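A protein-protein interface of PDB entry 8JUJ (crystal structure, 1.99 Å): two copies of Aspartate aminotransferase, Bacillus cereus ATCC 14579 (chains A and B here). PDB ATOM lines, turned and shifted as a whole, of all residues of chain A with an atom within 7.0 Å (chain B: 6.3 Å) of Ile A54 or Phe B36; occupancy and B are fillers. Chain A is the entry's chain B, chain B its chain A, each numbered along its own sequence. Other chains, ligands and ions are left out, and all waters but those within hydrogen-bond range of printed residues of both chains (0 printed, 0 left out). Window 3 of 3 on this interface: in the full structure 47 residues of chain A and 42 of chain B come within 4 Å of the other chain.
Among the printed residues, pairs that only touch across the chains: Pro A53 with Glu B37, Ile A54 with Phe B36, Phe A55 with Val B38 and Gly A56 with Asn B233.
The backbone carbonyl oxygen (O) of Met B34 lies within hydrogen-bond range of the side-chain amide nitrogen (ND2) of Asn B233, 2.8 Å away.
The backbone carbonyl oxygen (O) of Phe B36 lies within hydrogen-bond range of the side-chain amide nitrogen (ND2) of Asn B233.
The backbone carbonyl oxygen of Ile A54 is in hydrogen-bond range of the guanidinium group of Arg A49 (2.8 Å).
Printed residues of chain B within 4 Å of Pro A53: Glu B37 (3.4 Å) and Val B38 (2.8 Å).
Ile A54 touches just one residue of chain B: Phe B36.
Printed residues of chain B within 4 Å of Phe A55: Val B38 and Asn B233.
Phe B36 touches one residue of chain A.
Printed residues of chain A within 4 Å of Glu B37: Pro A53.
Of the printed residues of chain A, Val B38 touches Pro A53 and Phe A55.
Printed residues of chain A within 4 Å of Asn B233: Phe A55 and Gly A56.
The nearest residue of chain B that does not touch Ile A54 is Glu B37 (4.05 Å).
No position is printed for both chains.
Of the 17 printed residues of chain B, 4 touch a printed residue of chain A.
Hydrophobic or aromatic side chains of chain A within 4 Å of the printed part of chain B: Pro A53, Ile A54 and Phe A55.
The backbone carbonyl oxygen (O) of Pro A53 is in hydrogen-bond range of the backbone NH (N) of Val B38, at 2.8 Å.
N of Phe A55 lies close to O of Asn B233 (3.5 Å).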
ATOM      1  N   ARG A  49      -5.808  23.545  10.916  1.00  0.00           N
ATOM      2  CA  ARG A  49      -7.151  24.090  11.175  1.00  0.00           C
ATOM      3  C   ARG A  49      -7.689  23.516  12.492  1.00  0.00           C
ATOM      4  O   ARG A  49      -8.305  24.278  13.262  1.00  0.00           O
ATOM      5  CB  ARG A  49      -8.073  23.753   9.999  1.00  0.00           C
ATOM      6  CG  ARG A  49      -9.472  24.343  10.133  1.00  0.00           C
ATOM      7  CD  ARG A  49      -9.417  25.845  10.323  1.00  0.00           C
ATOM      8  NE  ARG A  49     -10.687  26.466  10.641  1.00  0.00           N
ATOM      9  CZ  ARG A  49     -11.265  26.490  11.832  1.00  0.00           C
ATOM     10  NH1 ARG A  49     -10.732  25.864  12.873  1.00  0.00           N
ATOM     11  NH2 ARG A  49     -12.406  27.128  11.975  1.00  0.00           N
ATOM     12  N   ILE A  50      -7.475  22.229  12.769  1.00  0.00           N
ATOM     13  CA  ILE A  50      -7.986  21.609  14.034  1.00  0.00           C
ATOM     14  C   ILE A  50      -7.299  22.264  15.247  1.00  0.00           C
ATOM     15  O   ILE A  50      -7.914  22.286  16.323  1.00  0.00           O
ATOM     16  CB  ILE A  50      -7.857  20.073  14.024  1.00  0.00           C
ATOM     17  CG1 ILE A  50      -8.799  19.462  12.984  1.00  0.00           C
ATOM     18  CG2 ILE A  50      -8.121  19.498  15.410  1.00  0.00           C
ATOM     19  CD1 ILE A  50      -8.666  17.968  12.802  1.00  0.00           C
ATOM     20  N   GLU A  51      -6.104  22.836  15.089  1.00  0.00           N
ATOM     21  CA  GLU A  51      -5.361  23.483  16.212  1.00  0.00           C
ATOM     22  C   GLU A  51      -5.994  24.834  16.583  1.00  0.00           C
ATOM     23  O   GLU A  51      -5.571  25.414  17.583  1.00  0.00           O
ATOM     24  CB  GLU A  51      -3.882  23.671  15.865  1.00  0.00           C
ATOM     25  CG  GLU A  51      -2.991  22.569  16.422  1.00  0.00           C
ATOM     26  CD  GLU A  51      -1.844  22.222  15.495  1.00  0.00           C
ATOM     27  OE1 GLU A  51      -1.341  23.160  14.807  1.00  0.00           O
ATOM     28  OE2 GLU A  51      -1.479  21.015  15.434  1.00  0.00           O
ATOM     29  N   HIS A  52      -6.948  25.341  15.803  1.00  0.00           N
ATOM     30  CA  HIS A  52      -7.767  26.526  16.171  1.00  0.00           C
ATOM     31  C   HIS A  52      -9.162  26.024  16.525  1.00  0.00           C
ATOM     32  O   HIS A  52     -10.012  25.924  15.649  1.00  0.00           O
ATOM     33  CB  HIS A  52      -7.776  27.554  15.037  1.00  0.00           C
ATOM     34  CG  HIS A  52      -8.284  28.878  15.474  1.00  0.00           C
ATOM     35  ND1 HIS A  52      -9.216  29.007  16.487  1.00  0.00           N
ATOM     36  CD2 HIS A  52      -7.998  30.128  15.050  1.00  0.00           C
ATOM     37  CE1 HIS A  52      -9.480  30.282  16.676  1.00  0.00           C
ATOM     38  NE2 HIS A  52      -8.754  30.991  15.797  1.00  0.00           N
ATOM     39  N   PRO A  53      -9.432  25.658  17.796  1.00  0.00           N
ATOM     40  CA  PRO A  53     -10.556  24.779  18.108  1.00  0.00           C
ATOM     41  C   PRO A  53     -11.904  25.502  18.259  1.00  0.00           C
ATOM     42  O   PRO A  53     -12.594  25.289  19.247  1.00  0.00           O
ATOM     43  CB  PRO A  53     -10.067  24.152  19.415  1.00  0.00           C
ATOM     44  CG  PRO A  53      -9.372  25.304  20.117  1.00  0.00           C
ATOM     45  CD  PRO A  53      -8.677  26.057  18.999  1.00  0.00           C
ATOM     46  N   ILE A  54     -12.226  26.341  17.280  1.00  0.00           N
ATOM     47  CA  ILE A  54     -13.598  26.851  16.982  1.00  0.00           C
ATOM     48  C   ILE A  54     -13.959  26.416  15.545  1.00  0.00           C
ATOM     49  O   ILE A  54     -13.088  26.500  14.659  1.00  0.00           O
ATOM     50  CB  ILE A  54     -13.682  28.375  17.200  1.00  0.00           C
ATOM     51  CG1 ILE A  54     -12.668  29.147  16.341  1.00  0.00           C
ATOM     52  CG2 ILE A  54     -13.517  28.676  18.692  1.00  0.00           C
ATOM     53  CD1 ILE A  54     -13.254  30.305  15.514  1.00  0.00           C
ATOM     54  N   PHE A  55     -15.182  25.910  15.364  1.00  0.00           N
ATOM     55  CA  PHE A  55     -15.708  25.323  14.099  1.00  0.00           C
ATOM     56  C   PHE A  55     -17.126  25.861  13.831  1.00  0.00           C
ATOM     57  O   PHE A  55     -18.075  25.087  13.637  1.00  0.00           O
ATOM     58  CB  PHE A  55     -15.685  23.796  14.191  1.00  0.00           C
ATOM     59  CG  PHE A  55     -14.323  23.238  14.513  1.00  0.00           C
ATOM     60  CD1 PHE A  55     -13.284  23.328  13.600  1.00  0.00           C
ATOM     61  CD2 PHE A  55     -14.060  22.692  15.762  1.00  0.00           C
ATOM     62  CE1 PHE A  55     -12.011  22.869  13.924  1.00  0.00           C
ATOM     63  CE2 PHE A  55     -12.795  22.199  16.071  1.00  0.00           C
ATOM     64  CZ  PHE A  55     -11.772  22.302  15.152  1.00  0.00           C
ATOM     65  N   GLY A  56     -17.279  27.175  13.877  1.00  0.00           N
ATOM     66  CA  GLY A  56     -18.559  27.852  13.594  1.00  0.00           C
ATOM     67  C   GLY A  56     -18.649  28.171  12.116  1.00  0.00           C
ATOM     68  O   GLY A  56     -17.799  27.670  11.361  1.00  0.00           O
ATOM     69  N   THR A  58     -18.289  29.698   8.567  1.00  0.00           N
ATOM     70  CA  THR A  58     -17.102  30.279   7.916  1.00  0.00           C
ATOM     71  C   THR A  58     -17.468  30.601   6.480  1.00  0.00           C
ATOM     72  O   THR A  58     -18.259  29.845   5.918  1.00  0.00           O
ATOM     73  CB  THR A  58     -15.906  29.328   7.994  1.00  0.00           C
ATOM     74  OG1 THR A  58     -15.838  28.590   6.776  1.00  0.00           O
ATOM     75  CG2 THR A  58     -16.000  28.390   9.175  1.00  0.00           C
ATOM     76  N   ILE A 267     -16.137  23.609   6.780  1.00  0.00           N
ATOM     77  CA  ILE A 267     -14.809  24.239   7.036  1.00  0.00           C
ATOM     78  C   ILE A 267     -13.692  23.481   6.313  1.00  0.00           C
ATOM     79  O   ILE A 267     -12.811  24.116   5.701  1.00  0.00           O
ATOM     80  CB  ILE A 267     -14.584  24.265   8.555  1.00  0.00           C
ATOM     81  CG1 ILE A 267     -15.428  25.365   9.179  1.00  0.00           C
ATOM     82  CG2 ILE A 267     -13.113  24.403   8.900  1.00  0.00           C
ATOM     83  CD1 ILE A 267     -15.585  25.258  10.685  1.00  0.00           C
ATOM     84  N   MET B  34     -21.442  30.698  19.286  1.00  0.00           N
ATOM     85  CA  MET B  34     -20.733  31.010  20.550  1.00  0.00           C
ATOM     86  C   MET B  34     -19.275  31.335  20.237  1.00  0.00           C
ATOM     87  O   MET B  34     -18.751  30.713  19.317  1.00  0.00           O
ATOM     88  CB  MET B  34     -20.771  29.795  21.477  1.00  0.00           C
ATOM     89  CG  MET B  34     -22.153  29.453  21.961  1.00  0.00           C
ATOM     90  SD  MET B  34     -22.187  27.980  23.060  1.00  0.00           S
ATOM     91  CE  MET B  34     -20.681  27.153  22.563  1.00  0.00           C
ATOM     92  N   ASP B  35     -18.652  32.231  21.009  1.00  0.00           N
ATOM     93  CA  ASP B  35     -17.186  32.483  21.019  1.00  0.00           C
ATOM     94  C   ASP B  35     -16.564  31.662  22.152  1.00  0.00           C
ATOM     95  O   ASP B  35     -15.915  32.254  23.012  1.00  0.00           O
ATOM     96  CB  ASP B  35     -16.845  33.958  21.265  1.00  0.00           C
ATOM     97  CG  ASP B  35     -17.396  34.952  20.256  1.00  0.00           C
ATOM     98  OD1 ASP B  35     -18.167  34.549  19.345  1.00  0.00           O
ATOM     99  OD2 ASP B  35     -17.062  36.138  20.403  1.00  0.00           O
ATOM    100  N   PHE B  36     -16.806  30.358  22.192  1.00  0.00           N
ATOM    101  CA  PHE B  36     -16.158  29.412  23.131  1.00  0.00           C
ATOM    102  C   PHE B  36     -15.508  28.286  22.325  1.00  0.00           C
ATOM    103  O   PHE B  36     -16.063  27.821  21.321  1.00  0.00           O
ATOM    104  CB  PHE B  36     -17.149  28.796  24.123  1.00  0.00           C
ATOM    105  CG  PHE B  36     -17.843  29.755  25.055  1.00  0.00           C
ATOM    106  CD1 PHE B  36     -17.122  30.601  25.879  1.00  0.00           C
ATOM    107  CD2 PHE B  36     -19.228  29.760  25.163  1.00  0.00           C
ATOM    108  CE1 PHE B  36     -17.764  31.460  26.760  1.00  0.00           C
ATOM    109  CE2 PHE B  36     -19.867  30.615  26.046  1.00  0.00           C
ATOM    110  CZ  PHE B  36     -19.137  31.473  26.836  1.00  0.00           C
ATOM    111  N   GLU B  37     -14.342  27.845  22.780  1.00  0.00           N
ATOM    112  CA  GLU B  37     -13.616  26.689  22.216  1.00  0.00           C
ATOM    113  C   GLU B  37     -14.506  25.453  22.320  1.00  0.00           C
ATOM    114  O   GLU B  37     -15.212  25.271  23.322  1.00  0.00           O
ATOM    115  CB  GLU B  37     -12.287  26.468  22.941  1.00  0.00           C
ATOM    116  CG  GLU B  37     -11.441  27.724  23.036  1.00  0.00           C
ATOM    117  CD  GLU B  37      -9.942  27.470  23.027  1.00  0.00           C
ATOM    118  OE1 GLU B  37      -9.189  28.378  22.613  1.00  0.00           O
ATOM    119  OE2 GLU B  37      -9.531  26.357  23.415  1.00  0.00           O
ATOM    120  N   VAL B  38     -14.476  24.649  21.270  1.00  0.00           N
ATOM    121  CA  VAL B  38     -15.094  23.304  21.181  1.00  0.00           C
ATOM    122  C   VAL B  38     -14.645  22.420  22.350  1.00  0.00           C
ATOM    123  O   VAL B  38     -13.527  22.522  22.840  1.00  0.00           O
ATOM    124  CB  VAL B  38     -14.701  22.797  19.777  1.00  0.00           C
ATOM    125  CG1 VAL B  38     -14.605  21.288  19.641  1.00  0.00           C
ATOM    126  CG2 VAL B  38     -15.616  23.413  18.733  1.00  0.00           C
ATOM    127  N   PHE B 232     -22.352  22.858  20.678  1.00  0.00           N
ATOM    128  CA  PHE B 232     -20.913  22.522  20.812  1.00  0.00           C
ATOM    129  C   PHE B 232     -20.060  23.411  19.907  1.00  0.00           C
ATOM    130  O   PHE B 232     -18.851  23.166  19.853  1.00  0.00           O
ATOM    131  CB  PHE B 232     -20.755  21.028  20.557  1.00  0.00           C
ATOM    132  CG  PHE B 232     -21.500  20.187  21.554  1.00  0.00           C
ATOM    133  CD1 PHE B 232     -21.096  20.150  22.883  1.00  0.00           C
ATOM    134  CD2 PHE B 232     -22.598  19.437  21.175  1.00  0.00           C
ATOM    135  CE1 PHE B 232     -21.754  19.344  23.801  1.00  0.00           C
ATOM    136  CE2 PHE B 232     -23.268  18.648  22.098  1.00  0.00           C
ATOM    137  CZ  PHE B 232     -22.855  18.614  23.415  1.00  0.00           C
ATOM    138  N   ASN B 233     -20.657  24.404  19.235  1.00  0.00           N
ATOM    139  CA  ASN B 233     -19.919  25.384  18.394  1.00  0.00           C
ATOM    140  C   ASN B 233     -19.241  24.647  17.217  1.00  0.00           C
ATOM    141  O   ASN B 233     -18.065  24.863  16.964  1.00  0.00           O
ATOM    142  CB  ASN B 233     -18.930  26.201  19.232  1.00  0.00           C
ATOM    143  CG  ASN B 233     -18.498  27.500  18.573  1.00  0.00           C
ATOM    144  OD1 ASN B 233     -19.009  27.896  17.527  1.00  0.00           O
ATOM    145  ND2 ASN B 233     -17.559  28.199  19.181  1.00  0.00           N
ATOM    146  N   TRP B 283     -18.782  19.333  29.841  1.00  0.00           N
ATOM    147  CA  TRP B 283     -18.636  20.620  29.114  1.00  0.00           C
ATOM    148  C   TRP B 283     -20.014  21.265  28.926  1.00  0.00           C
ATOM    149  O   TRP B 283     -20.107  22.470  29.094  1.00  0.00           O
ATOM    150  CB  TRP B 283     -17.910  20.412  27.785  1.00  0.00           C
ATOM    151  CG  TRP B 283     -17.634  21.673  27.029  1.00  0.00           C
ATOM    152  CD1 TRP B 283     -16.479  22.396  27.029  1.00  0.00           C
ATOM    153  CD2 TRP B 283     -18.537  22.361  26.137  1.00  0.00           C
ATOM    154  NE1 TRP B 283     -16.596  23.470  26.191  1.00  0.00           N
ATOM    155  CE2 TRP B 283     -17.843  23.470  25.627  1.00  0.00           C
ATOM    156  CE3 TRP B 283     -19.843  22.119  25.695  1.00  0.00           C
ATOM    157  CZ2 TRP B 283     -18.416  24.338  24.699  1.00  0.00           C
ATOM    158  CZ3 TRP B 283     -20.421  22.991  24.800  1.00  0.00           C
ATOM    159  CH2 TRP B 283     -19.710  24.080  24.313  1.00  0.00           C
ATOM    160  N   ILE B 287     -21.323  24.833  30.381  1.00  0.00           N
ATOM    161  CA  ILE B 287     -21.631  25.966  29.449  1.00  0.00           C
ATOM    162  C   ILE B 287     -23.011  26.526  29.791  1.00  0.00           C
ATOM    163  O   ILE B 287     -23.168  27.761  29.759  1.00  0.00           O
ATOM    164  CB  ILE B 287     -21.496  25.545  27.970  1.00  0.00           C
ATOM    165  CG1 ILE B 287     -20.046  25.671  27.503  1.00  0.00           C
ATOM    166  CG2 ILE B 287     -22.416  26.344  27.068  1.00  0.00           C
ATOM    167  CD1 ILE B 287     -19.550  27.095  27.366  1.00  0.00           C
ATOM    168  N   TYR B 290     -22.687  28.932  32.664  1.00  0.00           N
ATOM    169  CA  TYR B 290     -21.929  30.162  32.305  1.00  0.00           C
ATOM    170  C   TYR B 290     -22.824  31.103  31.484  1.00  0.00           C
ATOM    171  O   TYR B 290     -22.882  32.324  31.721  1.00  0.00           O
ATOM    172  CB  TYR B 290     -20.673  29.763  31.536  1.00  0.00           C
ATOM    173  CG  TYR B 290     -19.662  30.866  31.456  1.00  0.00           C
ATOM    174  CD1 TYR B 290     -19.732  31.808  30.452  1.00  0.00           C
ATOM    175  CD2 TYR B 290     -18.680  31.000  32.418  1.00  0.00           C
ATOM    176  CE1 TYR B 290     -18.820  32.839  30.371  1.00  0.00           C
ATOM    177  CE2 TYR B 290     -17.753  32.026  32.348  1.00  0.00           C
ATOM    178  CZ  TYR B 290     -17.822  32.946  31.318  1.00  0.00           C
ATOM    179  OH  TYR B 290     -16.930  33.972  31.219  1.00  0.00           O
ATOM    180  N   ILE B 291     -23.536  30.546  30.503  1.00  0.00           N
ATOM    181  CA  ILE B 291     -24.437  31.370  29.650  1.00  0.00           C
ATOM    182  C   ILE B 291     -25.574  31.958  30.506  1.00  0.00           C
ATOM    183  O   ILE B 291     -25.808  33.165  30.410  1.00  0.00           O
ATOM    184  CB  ILE B 291     -24.900  30.565  28.420  1.00  0.00           C
ATOM    185  CG1 ILE B 291     -23.709  30.369  27.469  1.00  0.00           C
ATOM    186  CG2 ILE B 291     -26.076  31.238  27.729  1.00  0.00           C
ATOM    187  CD1 ILE B 291     -23.910  29.270  26.467  1.00  0.00           C
ATOM    188  N   ASN B 294     -24.274  34.743  32.410  1.00  0.00           N
ATOM    189  CA  ASN B 294     -24.146  35.877  31.462  1.00  0.00           C
ATOM    190  C   ASN B 294     -25.535  36.500  31.283  1.00  0.00           C
ATOM    191  O   ASN B 294     -25.629  37.717  31.361  1.00  0.00           O
ATOM    192  CB  ASN B 294     -23.563  35.473  30.109  1.00  0.00           C
ATOM    193  CG  ASN B 294     -22.049  35.393  30.049  1.00  0.00           C
ATOM    194  OD1 ASN B 294     -21.324  35.692  31.006  1.00  0.00           O
ATOM    195  ND2 ASN B 294     -21.558  34.962  28.903  1.00  0.00           N
ATOM    196  N   ILE B 364     -24.810  36.463  23.662  1.00  0.00           N
ATOM    197  CA  ILE B 364     -24.195  36.487  25.033  1.00  0.00           C
ATOM    198  C   ILE B 364     -23.425  35.195  25.274  1.00  0.00           C
ATOM    199  O   ILE B 364     -23.049  35.014  26.405  1.00  0.00           O
ATOM    200  CB  ILE B 364     -25.223  36.721  26.158  1.00  0.00           C
ATOM    201  CG1 ILE B 364     -26.255  35.589  26.265  1.00  0.00           C
ATOM    202  CG2 ILE B 364     -25.845  38.093  26.024  1.00  0.00           C
ATOM    203  CD1 ILE B 364     -27.319  35.774  27.350  1.00  0.00           C
ATOM    204  N   GLY B 365     -23.271  34.329  24.256  1.00  0.00           N
ATOM    205  CA  GLY B 365     -22.461  33.097  24.279  1.00  0.00           C
ATOM    206  C   GLY B 365     -20.977  33.397  24.136  1.00  0.00           C
ATOM    207  O   GLY B 365     -20.358  32.943  23.149  1.00  0.00           O
ATOM    208  N   CYS B 366     -20.414  34.136  25.092  1.00  0.00           N
ATOM    209  CA  CYS B 366     -19.016  34.642  25.046  1.00  0.00           C
ATOM    210  C   CYS B 366     -18.474  34.744  26.463  1.00  0.00           C
ATOM    211  O   CYS B 366     -19.244  34.694  27.415  1.00  0.00           O
ATOM    212  CB  CYS B 366     -18.944  35.997  24.343  1.00  0.00           C
ATOM    213  SG  CYS B 366     -20.008  37.264  25.087  1.00  0.00           S
ATOM    214  N   PRO B 367     -17.135  34.879  26.627  1.00  0.00           N
ATOM    215  CA  PRO B 367     -16.538  35.207  27.921  1.00  0.00           C
ATOM    216  C   PRO B 367     -17.182  36.440  28.564  1.00  0.00           C
ATOM    217  O   PRO B 367     -17.434  37.388  27.865  1.00  0.00           O
ATOM    218  CB  PRO B 367     -15.066  35.509  27.589  1.00  0.00           C
ATOM    219  CG  PRO B 367     -14.802  34.716  26.326  1.00  0.00           C
ATOM    220  CD  PRO B 367     -16.123  34.744  25.567  1.00  0.00           C
ATOM    221  N   ARG B 368     -17.422  36.379  29.877  1.00  0.00           N
ATOM    222  CA  ARG B 368     -17.995  37.489  30.685  1.00  0.00           C
ATOM    223  C   ARG B 368     -17.321  38.823  30.358  1.00  0.00           C
ATOM    224  O   ARG B 368     -18.025  39.836  30.347  1.00  0.00           O
ATOM    225  CB  ARG B 368     -17.843  37.247  32.188  1.00  0.00           C
ATOM    226  CG  ARG B 368     -18.274  38.444  33.025  1.00  0.00           C
ATOM    227  CD  ARG B 368     -19.736  38.814  32.809  1.00  0.00           C
ATOM    228  NE  ARG B 368     -20.515  37.625  33.127  1.00  0.00           N
ATOM    229  CZ  ARG B 368     -20.873  37.271  34.355  1.00  0.00           C
ATOM    230  NH1 ARG B 368     -20.589  38.068  35.369  1.00  0.00           N
ATOM    231  NH2 ARG B 368     -21.549  36.153  34.558  1.00  0.00           N
